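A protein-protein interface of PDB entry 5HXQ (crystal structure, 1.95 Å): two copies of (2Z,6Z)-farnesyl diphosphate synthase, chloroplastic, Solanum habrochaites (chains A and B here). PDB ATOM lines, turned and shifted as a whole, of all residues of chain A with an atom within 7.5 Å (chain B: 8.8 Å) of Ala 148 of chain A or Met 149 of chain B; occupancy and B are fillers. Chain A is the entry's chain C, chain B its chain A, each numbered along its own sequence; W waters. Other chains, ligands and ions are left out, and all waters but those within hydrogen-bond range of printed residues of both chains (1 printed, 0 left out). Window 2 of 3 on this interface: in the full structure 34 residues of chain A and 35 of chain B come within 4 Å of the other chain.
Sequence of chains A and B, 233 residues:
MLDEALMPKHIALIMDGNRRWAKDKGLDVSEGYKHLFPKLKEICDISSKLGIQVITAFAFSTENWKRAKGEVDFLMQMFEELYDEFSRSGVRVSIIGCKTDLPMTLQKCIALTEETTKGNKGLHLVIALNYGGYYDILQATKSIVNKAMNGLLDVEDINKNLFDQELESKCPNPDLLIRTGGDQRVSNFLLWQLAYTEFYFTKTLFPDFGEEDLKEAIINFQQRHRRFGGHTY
The side-chain sulfur (SD) of Met 149 of chain B is in hydrogen-bond range of the backbone NH (N) of Met 149 of chain A (3.7 Å). The backbone carbonyl oxygen of Ala 148 of chain A lies close to the side-chain sulfur of Met 149 of chain B, 3.5 Å away.
The backbone carbonyl oxygen of Lys 142 of chain B sits at hydrogen-bond distance from the side-chain amide nitrogen of Asn 146 of chain B (3.2 Å). O of Asn 146 of chain B sits close to OD1 of Asn 150 of chain B (3.0 Å). The backbone carbonyl oxygen of Lys 142 of chain A lies close to the side-chain amide nitrogen of Asn 146 of chain A (3.4 Å). The backbone carbonyl oxygen (O) of Asn 146 of chain A sits close to the side-chain amide nitrogen (ND2) of Asn 150 of chain A, at 3.3 Å.
Among the printed residues, merely in contact across the chains: Lys 142 of chain A with Val 155 of chain B (3.5 Å), Val 145 of chain A with Val 145 of chain B (3.7 Å), Val 145 of chain A with Ala 148 of chain B (3.7 Å), Val 145 of chain A with Val 155 of chain B (3.9 Å), Asn 146 of chain A with Val 155 of chain B (3.5 Å), Ala 148 of chain A with Val 145 of chain B (3.7 Å), Met 149 of chain A with Ala 148 of chain B (3.98 Å), Met 149 of chain A with Val 155 of chain B (3.6 Å), Val 155 of chain A with Val 145 of chain B (3.6 Å), Val 155 of chain A with Asn 146 of chain B (3.3 Å), Ile 158 of chain A with Lys 142 of chain B (3.5 Å) and Ile 158 of chain A with Val 145 of chain B (3.7 Å).
Ala 148 of chain A touches just these residues of chain B: Val 145 (3.7 Å) and Met 149 (3.4 Å). Printed residues of chain A within 4 Å of Lys 142 of chain B: Ile 158 (3.5 Å). Printed residues of chain A within 4 Å of Ala 148 of chain B: Val 145 and Met 149. Printed residues of chain A within 4 Å of Met 149 of chain B: Ala 148 (3.4 Å) and Met 149 (3.7 Å).
Of the 15 printed residues of chain B, 6 touch a printed residue of chain A. Hydrophobic or aromatic side chains of chain B that line the printed part of chain A: Val 145, Ala 148, Met 149 and Val 155. Of the 15 printed residues of chain A, 7 touch a printed residue of chain B. Among the printed residues, no Asp or Glu carboxylate lies within 4 Å of a Lys or Arg side-chain nitrogen of the other chain.
Lys 142 of chain A touches Val 155 of chain B, but with the chains exchanged Val 155 of chain A does not touch Lys 142 of chain B (4.1 Å). Val 145 of chain A touches Ala 148 of chain B, and with the chains exchanged Ala 148 of chain A touches Val 145 of chain B. Ala 148 of chain A touches Met 149 of chain B, and with the chains exchanged Met 149 of chain A touches Ala 148 of chain B. Met 149 of chain A touches its own counterpart, Met 149 of chain B. Of the 14 pairs that touch across the chains among the printed residues, 10 have their exchanged pair printed and touching as well.
Water W1 lies within hydrogen-bond range of the backbone carbonyl oxygen of Ile 158 of chain A and the side-chain amino group of Lys 142 of chain B.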
ATOM      1  N   LYS A 142      25.744  17.379   3.045  1.00  0.00           N
ATOM      2  CA  LYS A 142      25.812  17.856   1.657  1.00  0.00           C
ATOM      3  C   LYS A 142      24.463  18.278   1.131  1.00  0.00           C
ATOM      4  O   LYS A 142      24.374  19.247   0.390  1.00  0.00           O
ATOM      5  CB  LYS A 142      26.388  16.788   0.738  1.00  0.00           C
ATOM      6  CG  LYS A 142      27.891  16.623   0.849  1.00  0.00           C
ATOM      7  CD  LYS A 142      28.351  15.550  -0.118  1.00  0.00           C
ATOM      8  CE  LYS A 142      29.833  15.286  -0.030  1.00  0.00           C
ATOM      9  NZ  LYS A 142      30.199  14.082  -0.829  1.00  0.00           N
ATOM     10  N   SER A 143      23.414  17.549   1.505  1.00  0.00           N
ATOM     11  CA  SER A 143      22.056  17.913   1.115  1.00  0.00           C
ATOM     12  C   SER A 143      21.601  19.220   1.788  1.00  0.00           C
ATOM     13  O   SER A 143      21.018  20.087   1.135  1.00  0.00           O
ATOM     14  CB  SER A 143      21.094  16.745   1.385  1.00  0.00           C
ATOM     15  OG  SER A 143      19.739  17.149   1.283  1.00  0.00           O
ATOM     16  N   ILE A 144      21.892  19.384   3.073  1.00  0.00           N
ATOM     17  CA  ILE A 144      21.572  20.636   3.782  1.00  0.00           C
ATOM     18  C   ILE A 144      22.366  21.834   3.212  1.00  0.00           C
ATOM     19  O   ILE A 144      21.834  22.936   3.087  1.00  0.00           O
ATOM     20  CB  ILE A 144      21.818  20.501   5.302  1.00  0.00           C
ATOM     21  CG1 ILE A 144      20.809  19.510   5.910  1.00  0.00           C
ATOM     22  CG2 ILE A 144      21.711  21.854   6.005  1.00  0.00           C
ATOM     23  CD1 ILE A 144      21.189  19.025   7.295  1.00  0.00           C
ATOM     24  N   VAL A 145      23.624  21.617   2.858  1.00  0.00           N
ATOM     25  CA  VAL A 145      24.422  22.676   2.242  1.00  0.00           C
ATOM     26  C   VAL A 145      23.830  23.100   0.882  1.00  0.00           C
ATOM     27  O   VAL A 145      23.672  24.296   0.626  1.00  0.00           O
ATOM     28  CB  VAL A 145      25.905  22.267   2.120  1.00  0.00           C
ATOM     29  CG1 VAL A 145      26.663  23.230   1.207  1.00  0.00           C
ATOM     30  CG2 VAL A 145      26.546  22.215   3.505  1.00  0.00           C
ATOM     31  N   ASN A 146      23.473  22.131   0.036  1.00  0.00           N
ATOM     32  CA  ASN A 146      22.786  22.420  -1.234  1.00  0.00           C
ATOM     33  C   ASN A 146      21.537  23.284  -1.082  1.00  0.00           C
ATOM     34  O   ASN A 146      21.368  24.263  -1.807  1.00  0.00           O
ATOM     35  CB  ASN A 146      22.399  21.127  -1.959  1.00  0.00           C
ATOM     36  CG  ASN A 146      23.591  20.408  -2.551  1.00  0.00           C
ATOM     37  OD1 ASN A 146      24.674  20.978  -2.686  1.00  0.00           O
ATOM     38  ND2 ASN A 146      23.398  19.144  -2.911  1.00  0.00           N
ATOM     39  N   LYS A 147      20.663  22.920  -0.149  1.00  0.00           N
ATOM     40  CA  LYS A 147      19.445  23.685   0.105  1.00  0.00           C
ATOM     41  C   LYS A 147      19.747  25.087   0.630  1.00  0.00           C
ATOM     42  O   LYS A 147      19.041  26.049   0.297  1.00  0.00           O
ATOM     43  CB  LYS A 147      18.541  22.945   1.093  1.00  0.00           C
ATOM     44  CG  LYS A 147      17.975  21.655   0.533  1.00  0.00           C
ATOM     45  CD  LYS A 147      17.210  20.851   1.564  1.00  0.00           C
ATOM     46  CE  LYS A 147      16.707  19.565   0.929  1.00  0.00           C
ATOM     47  NZ  LYS A 147      15.858  18.787   1.862  1.00  0.00           N
ATOM     48  N   ALA A 148      20.784  25.197   1.456  1.00  0.00           N
ATOM     49  CA  ALA A 148      21.175  26.483   2.030  1.00  0.00           C
ATOM     50  C   ALA A 148      21.584  27.464   0.926  1.00  0.00           C
ATOM     51  O   ALA A 148      21.099  28.597   0.877  1.00  0.00           O
ATOM     52  CB  ALA A 148      22.310  26.307   3.030  1.00  0.00           C
ATOM     53  N   MET A 149      22.459  27.009   0.039  1.00  0.00           N
ATOM     54  CA  MET A 149      22.971  27.858  -1.034  1.00  0.00           C
ATOM     55  C   MET A 149      21.913  28.200  -2.089  1.00  0.00           C
ATOM     56  O   MET A 149      22.057  29.194  -2.794  1.00  0.00           O
ATOM     57  CB  MET A 149      24.194  27.209  -1.679  1.00  0.00           C
ATOM     58  CG  MET A 149      25.357  27.060  -0.710  1.00  0.00           C
ATOM     59  SD  MET A 149      26.883  26.460  -1.456  1.00  0.00           S
ATOM     60  CE  MET A 149      26.356  24.962  -2.286  1.00  0.00           C
ATOM     61  N   ASN A 150      20.849  27.401  -2.185  1.00  0.00           N
ATOM     62  CA  ASN A 150      19.743  27.686  -3.096  1.00  0.00           C
ATOM     63  C   ASN A 150      18.576  28.402  -2.426  1.00  0.00           C
ATOM     64  O   ASN A 150      17.482  28.443  -2.985  1.00  0.00           O
ATOM     65  CB  ASN A 150      19.244  26.391  -3.741  1.00  0.00           C
ATOM     66  CG  ASN A 150      20.346  25.640  -4.457  1.00  0.00           C
ATOM     67  OD1 ASN A 150      21.438  26.170  -4.663  1.00  0.00           O
ATOM     68  ND2 ASN A 150      20.074  24.394  -4.830  1.00  0.00           N
ATOM     69  N   GLY A 151      18.799  28.947  -1.229  1.00  0.00           N
ATOM     70  CA  GLY A 151      17.789  29.741  -0.527  1.00  0.00           C
ATOM     71  C   GLY A 151      16.615  28.956   0.027  1.00  0.00           C
ATOM     72  O   GLY A 151      15.619  29.546   0.459  1.00  0.00           O
ATOM     73  N   LEU A 152      16.737  27.628   0.046  1.00  0.00           N
ATOM     74  CA  LEU A 152      15.641  26.747   0.457  1.00  0.00           C
ATOM     75  C   LEU A 152      15.618  26.494   1.968  1.00  0.00           C
ATOM     76  O   LEU A 152      14.614  26.031   2.490  1.00  0.00           O
ATOM     77  CB  LEU A 152      15.716  25.419  -0.295  1.00  0.00           C
ATOM     78  CG  LEU A 152      15.702  25.525  -1.823  1.00  0.00           C
ATOM     79  CD1 LEU A 152      15.914  24.164  -2.463  1.00  0.00           C
ATOM     80  CD2 LEU A 152      14.402  26.147  -2.310  1.00  0.00           C
ATOM     81  N   LEU A 153      16.718  26.779   2.661  1.00  0.00           N
ATOM     82  CA  LEU A 153      16.677  26.880   4.119  1.00  0.00           C
ATOM     83  C   LEU A 153      17.783  27.762   4.680  1.00  0.00           C
ATOM     84  O   LEU A 153      18.799  28.000   4.030  1.00  0.00           O
ATOM     85  CB  LEU A 153      16.690  25.491   4.778  1.00  0.00           C
ATOM     86  CG  LEU A 153      17.856  24.545   4.499  1.00  0.00           C
ATOM     87  CD1 LEU A 153      19.121  24.987   5.226  1.00  0.00           C
ATOM     88  CD2 LEU A 153      17.469  23.125   4.904  1.00  0.00           C
ATOM     89  N   ASP A 154      17.561  28.240   5.898  1.00  0.00           N
ATOM     90  CA  ASP A 154      18.492  29.116   6.589  1.00  0.00           C
ATOM     91  C   ASP A 154      19.292  28.288   7.589  1.00  0.00           C
ATOM     92  O   ASP A 154      18.809  27.262   8.080  1.00  0.00           O
ATOM     93  CB  ASP A 154      17.717  30.220   7.323  1.00  0.00           C
ATOM     94  CG  ASP A 154      16.651  30.886   6.444  1.00  0.00           C
ATOM     95  OD1 ASP A 154      17.005  31.428   5.367  1.00  0.00           O
ATOM     96  OD2 ASP A 154      15.457  30.863   6.830  1.00  0.00           O
ATOM     97  N   VAL A 155      20.508  28.738   7.893  1.00  0.00           N
ATOM     98  CA  VAL A 155      21.359  28.083   8.888  1.00  0.00           C
ATOM     99  C   VAL A 155      20.601  27.766  10.180  1.00  0.00           C
ATOM    100  O   VAL A 155      20.803  26.704  10.765  1.00  0.00           O
ATOM    101  CB  VAL A 155      22.614  28.935   9.198  1.00  0.00           C
ATOM    102  CG1 VAL A 155      23.271  28.521  10.511  1.00  0.00           C
ATOM    103  CG2 VAL A 155      23.618  28.836   8.058  1.00  0.00           C
ATOM    104  N   ILE A 158      18.620  24.498  10.873  1.00  0.00           N
ATOM    105  CA  ILE A 158      19.420  23.313  11.095  1.00  0.00           C
ATOM    106  C   ILE A 158      19.274  22.870  12.550  1.00  0.00           C
ATOM    107  O   ILE A 158      19.771  23.504  13.464  1.00  0.00           O
ATOM    108  CB  ILE A 158      20.885  23.562  10.741  1.00  0.00           C
ATOM    109  CG1 ILE A 158      20.994  23.875   9.241  1.00  0.00           C
ATOM    110  CG2 ILE A 158      21.721  22.335  11.057  1.00  0.00           C
ATOM    111  CD1 ILE A 158      22.324  24.464   8.835  1.00  0.00           C
ATOM    112  N   THR B 141      27.957  20.966  11.574  1.00  0.00           N
ATOM    113  CA  THR B 141      27.183  21.166  10.359  1.00  0.00           C
ATOM    114  C   THR B 141      26.890  22.643  10.089  1.00  0.00           C
ATOM    115  O   THR B 141      27.043  23.093   8.957  1.00  0.00           O
ATOM    116  CB  THR B 141      25.863  20.383  10.413  1.00  0.00           C
ATOM    117  OG1 THR B 141      26.162  18.997  10.575  1.00  0.00           O
ATOM    118  CG2 THR B 141      25.051  20.589   9.136  1.00  0.00           C
ATOM    119  N   LYS B 142      26.449  23.375  11.106  1.00  0.00           N
ATOM    120  CA  LYS B 142      26.172  24.806  10.951  1.00  0.00           C
ATOM    121  C   LYS B 142      27.420  25.566  10.516  1.00  0.00           C
ATOM    122  O   LYS B 142      27.348  26.479   9.696  1.00  0.00           O
ATOM    123  CB  LYS B 142      25.650  25.417  12.247  1.00  0.00           C
ATOM    124  CG  LYS B 142      24.199  25.111  12.550  1.00  0.00           C
ATOM    125  CD  LYS B 142      23.717  25.997  13.689  1.00  0.00           C
ATOM    126  CE  LYS B 142      22.578  25.359  14.464  1.00  0.00           C
ATOM    127  NZ  LYS B 142      22.309  26.116  15.722  1.00  0.00           N
ATOM    128  N   SER B 143      28.552  25.174  11.088  1.00  0.00           N
ATOM    129  CA  SER B 143      29.841  25.753  10.765  1.00  0.00           C
ATOM    130  C   SER B 143      30.232  25.490   9.304  1.00  0.00           C
ATOM    131  O   SER B 143      30.752  26.378   8.626  1.00  0.00           O
ATOM    132  CB  SER B 143      30.896  25.216  11.735  1.00  0.00           C
ATOM    133  OG  SER B 143      32.170  25.748  11.458  1.00  0.00           O
ATOM    134  N   ILE B 144      29.975  24.278   8.834  1.00  0.00           N
ATOM    135  CA  ILE B 144      30.237  23.897   7.457  1.00  0.00           C
ATOM    136  C   ILE B 144      29.311  24.637   6.487  1.00  0.00           C
ATOM    137  O   ILE B 144      29.732  25.037   5.396  1.00  0.00           O
ATOM    138  CB  ILE B 144      30.118  22.368   7.292  1.00  0.00           C
ATOM    139  CG1 ILE B 144      31.323  21.693   7.963  1.00  0.00           C
ATOM    140  CG2 ILE B 144      30.036  21.972   5.822  1.00  0.00           C
ATOM    141  CD1 ILE B 144      31.099  20.244   8.337  1.00  0.00           C
ATOM    142  N   VAL B 145      28.056  24.826   6.879  1.00  0.00           N
ATOM    143  CA  VAL B 145      27.099  25.534   6.032  1.00  0.00           C
ATOM    144  C   VAL B 145      27.520  26.994   5.885  1.00  0.00           C
ATOM    145  O   VAL B 145      27.521  27.537   4.786  1.00  0.00           O
ATOM    146  CB  VAL B 145      25.663  25.425   6.576  1.00  0.00           C
ATOM    147  CG1 VAL B 145      24.710  26.324   5.796  1.00  0.00           C
ATOM    148  CG2 VAL B 145      25.184  23.980   6.495  1.00  0.00           C
ATOM    149  N   ASN B 146      27.891  27.614   7.001  1.00  0.00           N
ATOM    150  CA  ASN B 146      28.334  29.006   7.010  1.00  0.00           C
ATOM    151  C   ASN B 146      29.538  29.274   6.128  1.00  0.00           C
ATOM    152  O   ASN B 146      29.603  30.303   5.465  1.00  0.00           O
ATOM    153  CB  ASN B 146      28.674  29.430   8.430  1.00  0.00           C
ATOM    154  CG  ASN B 146      27.452  29.818   9.222  1.00  0.00           C
ATOM    155  OD1 ASN B 146      26.478  30.325   8.667  1.00  0.00           O
ATOM    156  ND2 ASN B 146      27.498  29.592  10.531  1.00  0.00           N
ATOM    157  N   LYS B 147      30.496  28.359   6.159  1.00  0.00           N
ATOM    158  CA  LYS B 147      31.677  28.452   5.328  1.00  0.00           C
ATOM    159  C   LYS B 147      31.338  28.272   3.851  1.00  0.00           C
ATOM    160  O   LYS B 147      31.930  28.936   2.998  1.00  0.00           O
ATOM    161  CB  LYS B 147      32.712  27.417   5.758  1.00  0.00           C
ATOM    162  CG  LYS B 147      33.387  27.751   7.071  1.00  0.00           C
ATOM    163  CD  LYS B 147      34.372  26.674   7.480  1.00  0.00           C
ATOM    164  CE  LYS B 147      35.064  27.035   8.786  1.00  0.00           C
ATOM    165  NZ  LYS B 147      36.267  26.194   9.012  1.00  0.00           N
ATOM    166  N   ALA B 148      30.393  27.380   3.551  1.00  0.00           N
ATOM    167  CA  ALA B 148      29.903  27.208   2.183  1.00  0.00           C
ATOM    168  C   ALA B 148      29.181  28.459   1.703  1.00  0.00           C
ATOM    169  O   ALA B 148      29.342  28.867   0.552  1.00  0.00           O
ATOM    170  CB  ALA B 148      28.972  26.007   2.081  1.00  0.00           C
ATOM    171  N   MET B 149      28.388  29.057   2.588  1.00  0.00           N
ATOM    172  CA  MET B 149      27.617  30.253   2.256  1.00  0.00           C
ATOM    173  C   MET B 149      28.493  31.508   2.082  1.00  0.00           C
ATOM    174  O   MET B 149      28.048  32.481   1.473  1.00  0.00           O
ATOM    175  CB  MET B 149      26.530  30.504   3.309  1.00  0.00           C
ATOM    176  CG  MET B 149      25.467  29.415   3.376  1.00  0.00           C
ATOM    177  SD  MET B 149      24.189  29.531   2.107  1.00  0.00           S
ATOM    178  CE  MET B 149      22.936  30.449   3.004  1.00  0.00           C
ATOM    179  N   ASN B 150      29.718  31.491   2.612  1.00  0.00           N
ATOM    180  CA  ASN B 150      30.682  32.578   2.390  1.00  0.00           C
ATOM    181  C   ASN B 150      31.774  32.211   1.379  1.00  0.00           C
ATOM    182  O   ASN B 150      32.873  32.762   1.430  1.00  0.00           O
ATOM    183  CB  ASN B 150      31.360  32.980   3.707  1.00  0.00           C
ATOM    184  CG  ASN B 150      30.373  33.329   4.802  1.00  0.00           C
ATOM    185  OD1 ASN B 150      30.613  33.047   5.977  1.00  0.00           O
ATOM    186  ND2 ASN B 150      29.256  33.947   4.426  1.00  0.00           N
ATOM    187  N   GLY B 151      31.492  31.265   0.484  1.00  0.00           N
ATOM    188  CA  GLY B 151      32.452  30.861  -0.549  1.00  0.00           C
ATOM    189  C   GLY B 151      33.759  30.244  -0.073  1.00  0.00           C
ATOM    190  O   GLY B 151      34.678  30.044  -0.872  1.00  0.00           O
ATOM    191  N   LEU B 152      33.854  29.915   1.212  1.00  0.00           N
ATOM    192  CA  LEU B 152      35.088  29.361   1.770  1.00  0.00           C
ATOM    193  C   LEU B 152      35.240  27.859   1.521  1.00  0.00           C
ATOM    194  O   LEU B 152      36.318  27.312   1.723  1.00  0.00           O
ATOM    195  CB  LEU B 152      35.176  29.652   3.268  1.00  0.00           C
ATOM    196  CG  LEU B 152      35.290  31.132   3.638  1.00  0.00           C
ATOM    197  CD1 LEU B 152      35.022  31.343   5.123  1.00  0.00           C
ATOM    198  CD2 LEU B 152      36.656  31.679   3.242  1.00  0.00           C
ATOM    199  N   LEU B 153      34.176  27.185   1.097  1.00  0.00           N
ATOM    200  CA  LEU B 153      34.292  25.775   0.734  1.00  0.00           C
ATOM    201  C   LEU B 153      33.203  25.343  -0.224  1.00  0.00           C
ATOM    202  O   LEU B 153      32.134  25.948  -0.279  1.00  0.00           O
ATOM    203  CB  LEU B 153      34.301  24.879   1.982  1.00  0.00           C
ATOM    204  CG  LEU B 153      33.099  24.901   2.933  1.00  0.00           C
ATOM    205  CD1 LEU B 153      31.972  23.987   2.458  1.00  0.00           C
ATOM    206  CD2 LEU B 153      33.552  24.492   4.328  1.00  0.00           C
ATOM    207  N   ASP B 154      33.500  24.289  -0.976  1.00  0.00           N
ATOM    208  CA  ASP B 154      32.561  23.693  -1.913  1.00  0.00           C
ATOM    209  C   ASP B 154      31.972  22.423  -1.318  1.00  0.00           C
ATOM    210  O   ASP B 154      32.465  21.907  -0.317  1.00  0.00           O
ATOM    211  CB  ASP B 154      33.272  23.360  -3.227  1.00  0.00           C
ATOM    212  CG  ASP B 154      33.948  24.570  -3.846  1.00  0.00           C
ATOM    213  OD1 ASP B 154      33.257  25.595  -4.050  1.00  0.00           O
ATOM    214  OD2 ASP B 154      35.168  24.497  -4.128  1.00  0.00           O
ATOM    215  N   VAL B 155      30.938  21.910  -1.970  1.00  0.00           N
ATOM    216  CA  VAL B 155      30.239  20.703  -1.524  1.00  0.00           C
ATOM    217  C   VAL B 155      31.152  19.473  -1.651  1.00  0.00           C
ATOM    218  O   VAL B 155      31.009  18.490  -0.914  1.00  0.00           O
ATOM    219  CB  VAL B 155      28.921  20.518  -2.320  1.00  0.00           C
ATOM    220  CG1 VAL B 155      28.156  19.279  -1.868  1.00  0.00           C
ATOM    221  CG2 VAL B 155      28.043  21.760  -2.172  1.00  0.00           C
HETATM  222  O   HOH W   1      20.532  23.549  16.219  1.00  0.00           O
